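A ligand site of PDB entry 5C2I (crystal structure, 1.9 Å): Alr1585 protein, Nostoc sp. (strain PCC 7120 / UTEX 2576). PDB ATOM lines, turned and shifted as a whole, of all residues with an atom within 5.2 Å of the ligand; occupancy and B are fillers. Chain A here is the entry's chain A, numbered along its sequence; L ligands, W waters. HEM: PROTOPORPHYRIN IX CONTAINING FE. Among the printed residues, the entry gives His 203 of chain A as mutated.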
ATOM      1  N   GLU A 197      -9.422 -20.711  25.559  1.00  0.00           N
ATOM      2  CA  GLU A 197      -8.154 -20.705  24.818  1.00  0.00           C
ATOM      3  C   GLU A 197      -7.052 -20.714  25.899  1.00  0.00           C
ATOM      4  O   GLU A 197      -7.326 -20.581  27.098  1.00  0.00           O
ATOM      5  CB  GLU A 197      -8.099 -19.519  23.874  1.00  0.00           C
ATOM      6  CG  GLU A 197      -8.385 -18.166  24.505  1.00  0.00           C
ATOM      7  CD  GLU A 197      -7.268 -17.719  25.451  1.00  0.00           C
ATOM      8  OE1 GLU A 197      -6.089 -17.870  25.103  1.00  0.00           O
ATOM      9  OE2 GLU A 197      -7.567 -17.255  26.567  1.00  0.00           O
ATOM     10  N   PHE A 199      -4.756 -18.857  27.223  1.00  0.00           N
ATOM     11  CA  PHE A 199      -4.598 -17.831  28.253  1.00  0.00           C
ATOM     12  C   PHE A 199      -5.676 -17.900  29.322  1.00  0.00           C
ATOM     13  O   PHE A 199      -5.586 -17.200  30.330  1.00  0.00           O
ATOM     14  CB  PHE A 199      -4.538 -16.401  27.643  1.00  0.00           C
ATOM     15  CG  PHE A 199      -3.393 -16.171  26.702  1.00  0.00           C
ATOM     16  CD1 PHE A 199      -2.140 -16.704  26.915  1.00  0.00           C
ATOM     17  CD2 PHE A 199      -3.570 -15.337  25.595  1.00  0.00           C
ATOM     18  CE1 PHE A 199      -1.071 -16.420  26.060  1.00  0.00           C
ATOM     19  CE2 PHE A 199      -2.526 -15.047  24.728  1.00  0.00           C
ATOM     20  CZ  PHE A 199      -1.248 -15.590  24.966  1.00  0.00           C
ATOM     21  N   PHE A 201      -9.167 -17.733  28.910  1.00  0.00           N
ATOM     22  CA  PHE A 201     -10.422 -17.045  28.663  1.00  0.00           C
ATOM     23  C   PHE A 201     -11.389 -17.893  27.855  1.00  0.00           C
ATOM     24  O   PHE A 201     -11.022 -18.527  26.862  1.00  0.00           O
ATOM     25  CB  PHE A 201     -10.180 -15.724  27.915  1.00  0.00           C
ATOM     26  CG  PHE A 201      -9.378 -14.722  28.711  1.00  0.00           C
ATOM     27  CD1 PHE A 201      -8.006 -14.875  28.849  1.00  0.00           C
ATOM     28  CD2 PHE A 201     -10.004 -13.670  29.347  1.00  0.00           C
ATOM     29  CE1 PHE A 201      -7.257 -13.947  29.565  1.00  0.00           C
ATOM     30  CE2 PHE A 201      -9.265 -12.756  30.111  1.00  0.00           C
ATOM     31  CZ  PHE A 201      -7.900 -12.893  30.239  1.00  0.00           C
ATOM     32  N   VAL A 202     -12.633 -17.887  28.266  1.00  0.00           N
ATOM     33  CA  VAL A 202     -13.701 -18.544  27.498  1.00  0.00           C
ATOM     34  C   VAL A 202     -13.697 -18.004  26.079  1.00  0.00           C
ATOM     35  O   VAL A 202     -13.502 -16.801  25.860  1.00  0.00           O
ATOM     36  CB  VAL A 202     -15.066 -18.337  28.145  1.00  0.00           C
ATOM     37  CG1 VAL A 202     -16.155 -19.003  27.316  1.00  0.00           C
ATOM     38  CG2 VAL A 202     -15.053 -19.014  29.492  1.00  0.00           C
ATOM     39  N   HIS A 203     -13.881 -18.896  25.120  1.00  0.00           N
ATOM     40  CA  HIS A 203     -13.598 -18.590  23.721  1.00  0.00           C
ATOM     41  C   HIS A 203     -14.669 -19.131  22.833  1.00  0.00           C
ATOM     42  O   HIS A 203     -15.120 -20.283  23.028  1.00  0.00           O
ATOM     43  CB  HIS A 203     -12.235 -19.167  23.361  1.00  0.00           C
ATOM     44  CG  HIS A 203     -11.632 -18.546  22.141  1.00  0.00           C
ATOM     45  ND1 HIS A 203     -11.051 -19.293  21.149  1.00  0.00           N
ATOM     46  CD2 HIS A 203     -11.525 -17.268  21.741  1.00  0.00           C
ATOM     47  CE1 HIS A 203     -10.580 -18.500  20.208  1.00  0.00           C
ATOM     48  NE2 HIS A 203     -10.876 -17.265  20.530  1.00  0.00           N
ATOM     49  N   GLY A 204     -15.043 -18.336  21.819  1.00  0.00           N
ATOM     50  CA  GLY A 204     -16.091 -18.703  20.887  1.00  0.00           C
ATOM     51  C   GLY A 204     -17.442 -18.149  21.262  1.00  0.00           C
ATOM     52  O   GLY A 204     -18.441 -18.592  20.727  1.00  0.00           O
ATOM     53  N   VAL A 205     -17.485 -17.165  22.155  1.00  0.00           N
ATOM     54  CA  VAL A 205     -18.745 -16.665  22.680  1.00  0.00           C
ATOM     55  C   VAL A 205     -19.571 -15.914  21.598  1.00  0.00           C
ATOM     56  O   VAL A 205     -20.757 -16.199  21.385  1.00  0.00           O
ATOM     57  CB  VAL A 205     -18.524 -15.730  23.887  1.00  0.00           C
ATOM     58  CG1 VAL A 205     -19.845 -15.194  24.374  1.00  0.00           C
ATOM     59  CG2 VAL A 205     -17.769 -16.422  24.998  1.00  0.00           C
ATOM     60  N   SER A 206     -18.949 -14.921  20.949  1.00  0.00           N
ATOM     61  CA  SER A 206     -19.661 -14.037  20.013  1.00  0.00           C
ATOM     62  C   SER A 206     -19.416 -14.430  18.559  1.00  0.00           C
ATOM     63  O   SER A 206     -18.279 -14.301  18.038  1.00  0.00           O
ATOM     64  CB  SER A 206     -19.229 -12.593  20.227  1.00  0.00           C
ATOM     65  OG  SER A 206     -19.978 -11.746  19.385  1.00  0.00           O
ATOM     66  N   LEU A 259      -1.288 -19.986  15.596  1.00  0.00           N
ATOM     67  CA  LEU A 259      -0.930 -18.847  16.467  1.00  0.00           C
ATOM     68  C   LEU A 259      -0.424 -19.395  17.803  1.00  0.00           C
ATOM     69  O   LEU A 259      -1.202 -19.825  18.645  1.00  0.00           O
ATOM     70  CB  LEU A 259      -2.153 -17.941  16.633  1.00  0.00           C
ATOM     71  CG  LEU A 259      -2.753 -17.344  15.369  1.00  0.00           C
ATOM     72  CD1 LEU A 259      -3.934 -16.406  15.698  1.00  0.00           C
ATOM     73  CD2 LEU A 259      -1.708 -16.616  14.554  1.00  0.00           C
ATOM     74  N   GLN A 261       1.004 -19.291  21.523  1.00  0.00           N
ATOM     75  CA  GLN A 261       0.687 -18.452  22.665  1.00  0.00           C
ATOM     76  C   GLN A 261       1.661 -18.678  23.805  1.00  0.00           C
ATOM     77  O   GLN A 261       1.764 -19.778  24.309  1.00  0.00           O
ATOM     78  CB  GLN A 261      -0.739 -18.737  23.158  1.00  0.00           C
ATOM     79  CG  GLN A 261      -1.827 -18.386  22.187  1.00  0.00           C
ATOM     80  CD  GLN A 261      -3.190 -18.838  22.649  1.00  0.00           C
ATOM     81  OE1 GLN A 261      -3.715 -19.858  22.206  1.00  0.00           O
ATOM     82  NE2 GLN A 261      -3.769 -18.083  23.592  1.00  0.00           N
ATOM     83  N   VAL A 289      -8.571  -8.359  27.217  1.00  0.00           N
ATOM     84  CA  VAL A 289      -9.399  -9.150  26.332  1.00  0.00           C
ATOM     85  C   VAL A 289     -10.724  -8.500  25.995  1.00  0.00           C
ATOM     86  O   VAL A 289     -11.197  -8.635  24.865  1.00  0.00           O
ATOM     87  CB  VAL A 289      -9.637 -10.547  26.930  1.00  0.00           C
ATOM     88  CG1 VAL A 289     -10.673 -11.320  26.155  1.00  0.00           C
ATOM     89  CG2 VAL A 289      -8.319 -11.324  26.985  1.00  0.00           C
ATOM     90  N   ARG A 291     -13.227  -9.217  28.141  1.00  0.00           N
ATOM     91  CA  ARG A 291     -14.023 -10.071  29.010  1.00  0.00           C
ATOM     92  C   ARG A 291     -13.122 -10.648  30.090  1.00  0.00           C
ATOM     93  O   ARG A 291     -11.943 -10.874  29.889  1.00  0.00           O
ATOM     94  CB  ARG A 291     -14.663 -11.248  28.258  1.00  0.00           C
ATOM     95  CG  ARG A 291     -15.707 -10.901  27.225  1.00  0.00           C
ATOM     96  CD  ARG A 291     -16.067 -12.163  26.465  1.00  0.00           C
ATOM     97  NE  ARG A 291     -16.990 -11.920  25.395  1.00  0.00           N
ATOM     98  CZ  ARG A 291     -18.325 -12.006  25.478  1.00  0.00           C
ATOM     99  NH1 ARG A 291     -18.947 -12.289  26.625  1.00  0.00           N
ATOM    100  NH2 ARG A 291     -19.035 -11.769  24.397  1.00  0.00           N
ATOM    101  N   ASN A 312     -23.801 -12.430  25.771  1.00  0.00           N
ATOM    102  CA  ASN A 312     -23.361 -11.676  24.605  1.00  0.00           C
ATOM    103  C   ASN A 312     -24.219 -10.488  24.301  1.00  0.00           C
ATOM    104  O   ASN A 312     -24.083  -9.831  23.237  1.00  0.00           O
ATOM    105  CB  ASN A 312     -23.257 -12.587  23.369  1.00  0.00           C
ATOM    106  CG  ASN A 312     -22.272 -12.031  22.342  1.00  0.00           C
ATOM    107  OD1 ASN A 312     -21.236 -11.473  22.704  1.00  0.00           O
ATOM    108  ND2 ASN A 312     -22.635 -12.131  21.099  1.00  0.00           N
ATOM    109  N   PHE A 314     -24.777  -7.220  24.691  1.00  0.00           N
ATOM    110  CA  PHE A 314     -24.342  -5.921  25.060  1.00  0.00           C
ATOM    111  C   PHE A 314     -23.851  -5.187  23.864  1.00  0.00           C
ATOM    112  O   PHE A 314     -23.588  -5.781  22.792  1.00  0.00           O
ATOM    113  CB  PHE A 314     -23.225  -5.991  26.115  1.00  0.00           C
ATOM    114  CG  PHE A 314     -21.951  -6.649  25.630  1.00  0.00           C
ATOM    115  CD1 PHE A 314     -21.805  -8.010  25.676  1.00  0.00           C
ATOM    116  CD2 PHE A 314     -20.929  -5.883  25.102  1.00  0.00           C
ATOM    117  CE1 PHE A 314     -20.642  -8.617  25.197  1.00  0.00           C
ATOM    118  CE2 PHE A 314     -19.776  -6.475  24.635  1.00  0.00           C
ATOM    119  CZ  PHE A 314     -19.624  -7.864  24.672  1.00  0.00           C
ATOM    120  N   HIS A 330      -9.399  -6.462  23.103  1.00  0.00           N
ATOM    121  CA  HIS A 330      -9.584  -7.354  21.960  1.00  0.00           C
ATOM    122  C   HIS A 330     -11.036  -7.394  21.403  1.00  0.00           C
ATOM    123  O   HIS A 330     -11.217  -7.285  20.172  1.00  0.00           O
ATOM    124  CB  HIS A 330      -9.091  -8.742  22.307  1.00  0.00           C
ATOM    125  CG  HIS A 330      -9.192  -9.745  21.185  1.00  0.00           C
ATOM    126  ND1 HIS A 330      -8.558  -9.572  19.975  1.00  0.00           N
ATOM    127  CD2 HIS A 330      -9.784 -10.962  21.136  1.00  0.00           C
ATOM    128  CE1 HIS A 330      -8.759 -10.648  19.227  1.00  0.00           C
ATOM    129  NE2 HIS A 330      -9.477 -11.498  19.917  1.00  0.00           N
ATOM    130  N   THR A 331     -12.028  -7.552  22.278  1.00  0.00           N
ATOM    131  CA  THR A 331     -13.418  -7.625  21.828  1.00  0.00           C
ATOM    132  C   THR A 331     -13.892  -6.364  21.174  1.00  0.00           C
ATOM    133  O   THR A 331     -14.623  -6.400  20.182  1.00  0.00           O
ATOM    134  CB  THR A 331     -14.421  -8.027  22.955  1.00  0.00           C
ATOM    135  OG1 THR A 331     -14.318  -7.117  24.026  1.00  0.00           O
ATOM    136  CG2 THR A 331     -14.159  -9.449  23.450  1.00  0.00           C
ATOM    137  N   THR A 334     -12.037  -5.907  17.646  1.00  0.00           N
ATOM    138  CA  THR A 334     -12.455  -6.841  16.618  1.00  0.00           C
ATOM    139  C   THR A 334     -13.948  -6.747  16.333  1.00  0.00           C
ATOM    140  O   THR A 334     -14.386  -7.092  15.226  1.00  0.00           O
ATOM    141  CB  THR A 334     -12.070  -8.284  16.961  1.00  0.00           C
ATOM    142  OG1 THR A 334     -12.673  -8.663  18.203  1.00  0.00           O
ATOM    143  CG2 THR A 334     -10.596  -8.460  17.043  1.00  0.00           C
ATOM    144  N   ASN A 335     -14.738  -6.301  17.309  1.00  0.00           N
ATOM    145  CA  ASN A 335     -16.152  -6.062  17.118  1.00  0.00           C
ATOM    146  C   ASN A 335     -16.550  -4.773  17.816  1.00  0.00           C
ATOM    147  O   ASN A 335     -16.857  -4.744  19.014  1.00  0.00           O
ATOM    148  CB  ASN A 335     -17.027  -7.203  17.600  1.00  0.00           C
ATOM    149  CG  ASN A 335     -18.506  -6.940  17.270  1.00  0.00           C
ATOM    150  OD1 ASN A 335     -18.852  -5.858  16.764  1.00  0.00           O
ATOM    151  ND2 ASN A 335     -19.374  -7.876  17.608  1.00  0.00           N
ATOM    152  N   ARG A 337     -19.091  -3.031  17.775  1.00  0.00           N
ATOM    153  CA  ARG A 337     -20.520  -2.939  18.080  1.00  0.00           C
ATOM    154  C   ARG A 337     -21.109  -1.527  17.928  1.00  0.00           C
ATOM    155  O   ARG A 337     -21.897  -1.056  18.779  1.00  0.00           O
ATOM    156  CB  ARG A 337     -20.818  -3.493  19.500  1.00  0.00           C
ATOM    157  CG  ARG A 337     -20.346  -4.923  19.650  1.00  0.00           C
ATOM    158  CD  ARG A 337     -20.803  -5.573  20.937  1.00  0.00           C
ATOM    159  NE  ARG A 337     -20.234  -6.912  21.015  1.00  0.00           N
ATOM    160  CZ  ARG A 337     -20.843  -8.022  21.444  1.00  0.00           C
ATOM    161  NH1 ARG A 337     -22.102  -8.017  21.884  1.00  0.00           N
ATOM    162  NH2 ARG A 337     -20.138  -9.160  21.474  1.00  0.00           N
ATOM    163  N   ILE A 362     -16.281 -12.015  11.132  1.00  0.00           N
ATOM    164  CA  ILE A 362     -15.781 -13.309  10.739  1.00  0.00           C
ATOM    165  C   ILE A 362     -16.457 -14.410  11.565  1.00  0.00           C
ATOM    166  O   ILE A 362     -16.910 -14.185  12.681  1.00  0.00           O
ATOM    167  CB  ILE A 362     -14.263 -13.429  10.940  1.00  0.00           C
ATOM    168  CG1 ILE A 362     -13.875 -13.135  12.396  1.00  0.00           C
ATOM    169  CG2 ILE A 362     -13.534 -12.474   9.978  1.00  0.00           C
ATOM    170  CD1 ILE A 362     -12.424 -13.532  12.715  1.00  0.00           C
ATOM    171  N   ARG A 364     -15.795 -17.807  13.365  1.00  0.00           N
ATOM    172  CA  ARG A 364     -14.592 -18.485  13.876  1.00  0.00           C
ATOM    173  C   ARG A 364     -14.871 -19.991  14.103  1.00  0.00           C
ATOM    174  O   ARG A 364     -15.959 -20.394  14.634  1.00  0.00           O
ATOM    175  CB  ARG A 364     -14.124 -17.798  15.145  1.00  0.00           C
ATOM    176  CG  ARG A 364     -13.588 -16.388  14.870  1.00  0.00           C
ATOM    177  CD  ARG A 364     -13.182 -15.654  16.141  1.00  0.00           C
ATOM    178  NE  ARG A 364     -14.402 -15.377  16.893  1.00  0.00           N
ATOM    179  CZ  ARG A 364     -14.525 -15.460  18.219  1.00  0.00           C
ATOM    180  NH1 ARG A 364     -13.493 -15.765  18.976  1.00  0.00           N
ATOM    181  NH2 ARG A 364     -15.688 -15.222  18.778  1.00  0.00           N
ATOM    182  N   LEU A 384      -3.324 -21.637  19.369  1.00  0.00           N
ATOM    183  CA  LEU A 384      -4.580 -21.680  18.737  1.00  0.00           C
ATOM    184  C   LEU A 384      -4.411 -21.977  17.270  1.00  0.00           C
ATOM    185  O   LEU A 384      -3.657 -21.288  16.560  1.00  0.00           O
ATOM    186  CB  LEU A 384      -5.305 -20.319  18.879  1.00  0.00           C
ATOM    187  CG  LEU A 384      -6.768 -20.283  18.435  1.00  0.00           C
ATOM    188  CD1 LEU A 384      -7.633 -21.029  19.451  1.00  0.00           C
ATOM    189  CD2 LEU A 384      -7.266 -18.843  18.259  1.00  0.00           C
ATOM    190  N   PHE A 386      -6.171 -21.140  14.457  1.00  0.00           N
ATOM    191  CA  PHE A 386      -7.178 -20.134  14.119  1.00  0.00           C
ATOM    192  C   PHE A 386      -7.754 -20.441  12.749  1.00  0.00           C
ATOM    193  O   PHE A 386      -7.020 -20.432  11.750  1.00  0.00           O
ATOM    194  CB  PHE A 386      -6.549 -18.729  14.135  1.00  0.00           C
ATOM    195  CG  PHE A 386      -7.497 -17.636  13.769  1.00  0.00           C
ATOM    196  CD1 PHE A 386      -8.303 -17.040  14.754  1.00  0.00           C
ATOM    197  CD2 PHE A 386      -7.628 -17.223  12.435  1.00  0.00           C
ATOM    198  CE1 PHE A 386      -9.172 -16.013  14.424  1.00  0.00           C
ATOM    199  CE2 PHE A 386      -8.504 -16.180  12.095  1.00  0.00           C
ATOM    200  CZ  PHE A 386      -9.294 -15.595  13.091  1.00  0.00           C
ATOM    201  N   PHE A 397     -11.519 -11.101   7.505  1.00  0.00           N
ATOM    202  CA  PHE A 397     -10.309 -11.321   8.303  1.00  0.00           C
ATOM    203  C   PHE A 397      -9.205 -10.271   8.050  1.00  0.00           C
ATOM    204  O   PHE A 397      -8.631  -9.745   9.014  1.00  0.00           O
ATOM    205  CB  PHE A 397      -9.707 -12.710   8.151  1.00  0.00           C
ATOM    206  CG  PHE A 397      -8.372 -12.824   8.776  1.00  0.00           C
ATOM    207  CD1 PHE A 397      -8.251 -13.025  10.152  1.00  0.00           C
ATOM    208  CD2 PHE A 397      -7.217 -12.639   8.043  1.00  0.00           C
ATOM    209  CE1 PHE A 397      -6.979 -13.021  10.749  1.00  0.00           C
ATOM    210  CE2 PHE A 397      -5.980 -12.655   8.635  1.00  0.00           C
ATOM    211  CZ  PHE A 397      -5.862 -12.844   9.993  1.00  0.00           C
ATOM    212  N   MET A 400     -10.082  -6.926   9.521  1.00  0.00           N
ATOM    213  CA  MET A 400     -10.139  -6.942  10.946  1.00  0.00           C
ATOM    214  C   MET A 400      -8.706  -6.854  11.532  1.00  0.00           C
ATOM    215  O   MET A 400      -8.461  -6.038  12.443  1.00  0.00           O
ATOM    216  CB  MET A 400     -10.866  -8.181  11.421  1.00  0.00           C
ATOM    217  CG  MET A 400     -11.135  -8.262  12.888  1.00  0.00           C
ATOM    218  SD  MET A 400     -12.145  -9.698  13.286  1.00  0.00           S
ATOM    219  CE  MET A 400     -13.727  -9.131  12.706  1.00  0.00           C
ATOM    220  N   GLN A 401      -7.799  -7.673  11.014  1.00  0.00           N
ATOM    221  CA  GLN A 401      -6.407  -7.654  11.500  1.00  0.00           C
ATOM    222  C   GLN A 401      -5.719  -6.332  11.148  1.00  0.00           C
ATOM    223  O   GLN A 401      -5.100  -5.679  12.015  1.00  0.00           O
ATOM    224  CB  GLN A 401      -5.619  -8.822  10.918  1.00  0.00           C
ATOM    225  CG  GLN A 401      -4.197  -8.948  11.454  1.00  0.00           C
ATOM    226  CD  GLN A 401      -4.122  -9.580  12.827  1.00  0.00           C
ATOM    227  OE1 GLN A 401      -4.682 -10.652  13.073  1.00  0.00           O
ATOM    228  NE2 GLN A 401      -3.453  -8.902  13.737  1.00  0.00           N
ATOM    229  N   LEU A 420      -3.725  -8.093  22.613  1.00  0.00           N
ATOM    230  CA  LEU A 420      -3.706  -9.525  22.435  1.00  0.00           C
ATOM    231  C   LEU A 420      -3.107  -9.961  21.108  1.00  0.00           C
ATOM    232  O   LEU A 420      -2.213 -10.787  21.084  1.00  0.00           O
ATOM    233  CB  LEU A 420      -5.154 -10.061  22.579  1.00  0.00           C
ATOM    234  CG  LEU A 420      -5.321 -11.552  22.761  1.00  0.00           C
ATOM    235  CD1 LEU A 420      -4.706 -12.004  24.084  1.00  0.00           C
ATOM    236  CD2 LEU A 420      -6.801 -11.946  22.705  1.00  0.00           C
ATOM    237  N   ILE A 421      -3.572  -9.370  19.977  1.00  0.00           N
ATOM    238  CA  ILE A 421      -3.190  -9.850  18.645  1.00  0.00           C
ATOM    239  C   ILE A 421      -2.617  -8.769  17.721  1.00  0.00           C
ATOM    240  O   ILE A 421      -2.209  -9.072  16.576  1.00  0.00           O
ATOM    241  CB  ILE A 421      -4.391 -10.498  17.893  1.00  0.00           C
ATOM    242  CG1 ILE A 421      -5.464  -9.461  17.575  1.00  0.00           C
ATOM    243  CG2 ILE A 421      -4.958 -11.651  18.632  1.00  0.00           C
ATOM    244  CD1 ILE A 421      -6.446  -9.846  16.479  1.00  0.00           C
ATOM    245  N   ILE A 448       1.570 -13.578  21.166  1.00  0.00           N
ATOM    246  CA  ILE A 448       1.095 -14.488  20.118  1.00  0.00           C
ATOM    247  C   ILE A 448       2.004 -14.373  18.908  1.00  0.00           C
ATOM    248  O   ILE A 448       2.357 -13.245  18.504  1.00  0.00           O
ATOM    249  CB  ILE A 448      -0.374 -14.138  19.778  1.00  0.00           C
ATOM    250  CG1 ILE A 448      -1.236 -14.463  21.004  1.00  0.00           C
ATOM    251  CG2 ILE A 448      -0.839 -14.878  18.544  1.00  0.00           C
ATOM    252  CD1 ILE A 448      -2.671 -13.930  20.954  1.00  0.00           C
HETATM  253  CHA HEM L   1     -13.194 -12.824  20.517  1.00  0.00           C
HETATM  254  CHB HEM L   1      -9.092 -14.770  22.159  1.00  0.00           C
HETATM  255  CHC HEM L   1      -7.127 -14.270  17.766  1.00  0.00           C
HETATM  256  CHD HEM L   1     -11.142 -12.095  16.241  1.00  0.00           C
HETATM  257  C1A HEM L   1     -12.238 -13.382  21.356  1.00  0.00           C
HETATM  258  C2A HEM L   1     -12.419 -13.643  22.750  1.00  0.00           C
HETATM  259  C3A HEM L   1     -11.274 -14.183  23.202  1.00  0.00           C
HETATM  260  C4A HEM L   1     -10.396 -14.284  22.097  1.00  0.00           C
HETATM  261  CMA HEM L   1     -10.957 -14.674  24.592  1.00  0.00           C
HETATM  262  CAA HEM L   1     -13.671 -13.374  23.596  1.00  0.00           C
HETATM  263  CBA HEM L   1     -14.738 -14.465  23.650  1.00  0.00           C
HETATM  264  CGA HEM L   1     -15.269 -14.706  22.268  1.00  0.00           C
HETATM  265  O1A HEM L   1     -16.174 -13.985  21.757  1.00  0.00           O
HETATM  266  O2A HEM L   1     -14.779 -15.635  21.609  1.00  0.00           O
HETATM  267  C1B HEM L   1      -8.223 -14.835  21.059  1.00  0.00           C
HETATM  268  C2B HEM L   1      -6.914 -15.411  21.115  1.00  0.00           C
HETATM  269  C3B HEM L   1      -6.376 -15.312  19.902  1.00  0.00           C
HETATM  270  C4B HEM L   1      -7.376 -14.602  19.096  1.00  0.00           C
HETATM  271  CMB HEM L   1      -6.300 -16.039  22.318  1.00  0.00           C
HETATM  272  CAB HEM L   1      -5.089 -15.793  19.345  1.00  0.00           C
HETATM  273  CBB HEM L   1      -4.384 -16.819  19.867  1.00  0.00           C
HETATM  274  C1C HEM L   1      -8.038 -13.572  16.952  1.00  0.00           C
HETATM  275  C2C HEM L   1      -7.793 -13.085  15.692  1.00  0.00           C
HETATM  276  C3C HEM L   1      -8.928 -12.446  15.269  1.00  0.00           C
HETATM  277  C4C HEM L   1      -9.872 -12.581  16.290  1.00  0.00           C
HETATM  278  CMC HEM L   1      -6.553 -13.253  14.855  1.00  0.00           C
HETATM  279  CAC HEM L   1      -9.192 -11.714  14.024  1.00  0.00           C
HETATM  280  CBC HEM L   1      -8.349 -11.053  13.279  1.00  0.00           C
HETATM  281  C1D HEM L   1     -12.044 -12.250  17.298  1.00  0.00           C
HETATM  282  C2D HEM L   1     -13.424 -11.799  17.177  1.00  0.00           C
HETATM  283  C3D HEM L   1     -13.988 -11.949  18.369  1.00  0.00           C
HETATM  284  C4D HEM L   1     -12.930 -12.564  19.201  1.00  0.00           C
HETATM  285  CMD HEM L   1     -14.122 -11.224  15.955  1.00  0.00           C
HETATM  286  CAD HEM L   1     -15.410 -11.656  18.727  1.00  0.00           C
HETATM  287  CBD HEM L   1     -15.658 -10.196  19.130  1.00  0.00           C
HETATM  288  CGD HEM L   1     -17.103  -9.990  19.425  1.00  0.00           C
HETATM  289  O1D HEM L   1     -17.378  -9.524  20.526  1.00  0.00           O
HETATM  290  O2D HEM L   1     -18.027 -10.269  18.582  1.00  0.00           O
HETATM  291  NA  HEM L   1     -10.967 -13.710  20.980  1.00  0.00           N
HETATM  292  NB  HEM L   1      -8.408 -14.321  19.892  1.00  0.00           N
HETATM  293  NC  HEM L   1      -9.280 -13.181  17.369  1.00  0.00           N
HETATM  294  ND  HEM L   1     -11.756 -12.633  18.538  1.00  0.00           N
HETATM  295 FE   HEM L   1     -10.120 -13.417  19.198  1.00  0.00          FE
HETATM  296  O   HOH W   1     -10.685 -15.537  18.399  1.00  0.00           O
HETATM  297  O   HOH W   2     -16.822 -10.995  13.863  1.00  0.00           O
HETATM  298  O   HOH W   3     -18.126 -11.909  16.171  1.00  0.00           O
HETATM  299  O   HOH W   4     -17.392  -6.671  21.010  1.00  0.00           O
HETATM  300  O   HOH W   5      -3.409 -13.048  13.457  1.00  0.00           O
HETATM  301  O   HOH W   6     -16.841 -11.359  22.489  1.00  0.00           O
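Glu 197 touches the ligand.
Phe 201 touches the ligand (CB to CMA, 3.6 Å).
Val 202 touches the ligand.
His 203 touches the ligand.
CD1 of Leu 259 touches CAB of the ligand, at 3.9 Å.
Gln 261 touches the ligand (NE2 to CMB, 3.5 Å).
CG1 of Val 289 touches CMA of the ligand (3.7 Å).
Arg 291 touches the ligand.
CG2 of Thr 331 touches CAA of the ligand, 3.96 Å away.
OG1 of Thr 334 touches C2D of the ligand, at 3.4 Å.
CD1 of Ile 362 touches CAC of the ligand, at 3.9 Å.
Leu 384 touches the ligand (CB to CBB, 3.8 Å).
CE1 of Phe 386 touches C2C of the ligand, 3.5 Å away.
CE1 of Phe 397 touches CBC of the ligand (3.5 Å).
Met 400 touches the ligand.
Gln 401 touches the ligand (OE1 to CMC, 3.7 Å).
CD2 of Leu 420 touches C1B of the ligand, 3.6 Å away.
Ile 421 touches the ligand (CG2 to CHC, 3.5 Å).
CD1 of Ile 448 touches CAB of the ligand, 3.5 Å away.
Hydrophobic or aromatic side chains that line the ligand: Phe 201, His 203, Val 205, Leu 259, Val 289, His 330, Ile 362, Leu 384, Phe 386, Phe 397, Met 400, Leu 420, Ile 421 and Ile 448.
Of the 29 residues printed, 26 come within 4 Å of the ligand.
Water W1 lies within hydrogen-bond range of NE2 of His 203 (2.8 Å) and NH1 of Arg 364 (2.9 Å).
Water W6 bridges an oxygen (O1D) of the ligand and the guanidinium group (NH2) of Arg 291.
Water W4 lies within hydrogen-bond range of O of Asn 335 (2.8 Å), NE of Arg 337 (2.9 Å), O1D of the ligand (2.9 Å) and O of Thr 331 (2.9 Å).
Water W3 bridges an oxygen (O2D) of the ligand and the backbone carbonyl oxygen (O) of Ser 206.
An iron atom (FE) of the ligand is bound by a ring nitrogen (NE2) of His 330, 2.1 Å away.
An oxygen (O1A) of the ligand lies within hydrogen-bond range of the backbone NH (N) of Ser 206 (3.0 Å).
An oxygen (O2D) of the ligand sits at hydrogen-bond distance from the side-chain hydroxyl (OG) of Ser 206 (2.6 Å).
The backbone NH of Gly 204 lies within hydrogen-bond range of an oxygen (O2A) of the ligand, at 2.7 Å.
The side-chain amide nitrogen of Asn 335 sits at hydrogen-bond distance from an oxygen (O2D) of the ligand, 2.9 Å away.
The guanidinium group (NH1) of Arg 364 is in salt-bridge range of an oxygen (O2A) of the ligand, at 2.9 Å.
The guanidinium group of Arg 337 is in salt-bridge range of an oxygen (O1D) of the ligand (2.9 Å).
N of Val 205 lies within hydrogen-bond range of O2A of the ligand.
The side-chain hydroxyl (OG1) of Thr 334 is in hydrogen-bond range of the backbone carbonyl oxygen (O) of His 330 (2.8 Å).
OG of Ser 206 sits at hydrogen-bond distance from ND2 of Asn 312 (3.2 Å).
OD1 of Asn 335 lies within hydrogen-bond range of N of Arg 337 (3.0 Å).
NH2 of Arg 337 is in hydrogen-bond range of OD1 of Asn 312, 2.8 Å away.
The guanidinium group (NH1) of Arg 337 sits at hydrogen-bond distance from the backbone carbonyl oxygen (O) of Phe 314, at 2.8 Å.
The backbone NH of Leu 384 lies within hydrogen-bond range of the side-chain amide oxygen of Gln 261.
NE2 of Gln 401 sits at hydrogen-bond distance from O of Ile 421, at 3.1 Å.
N of Leu 259 is in hydrogen-bond range of O of Leu 384.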
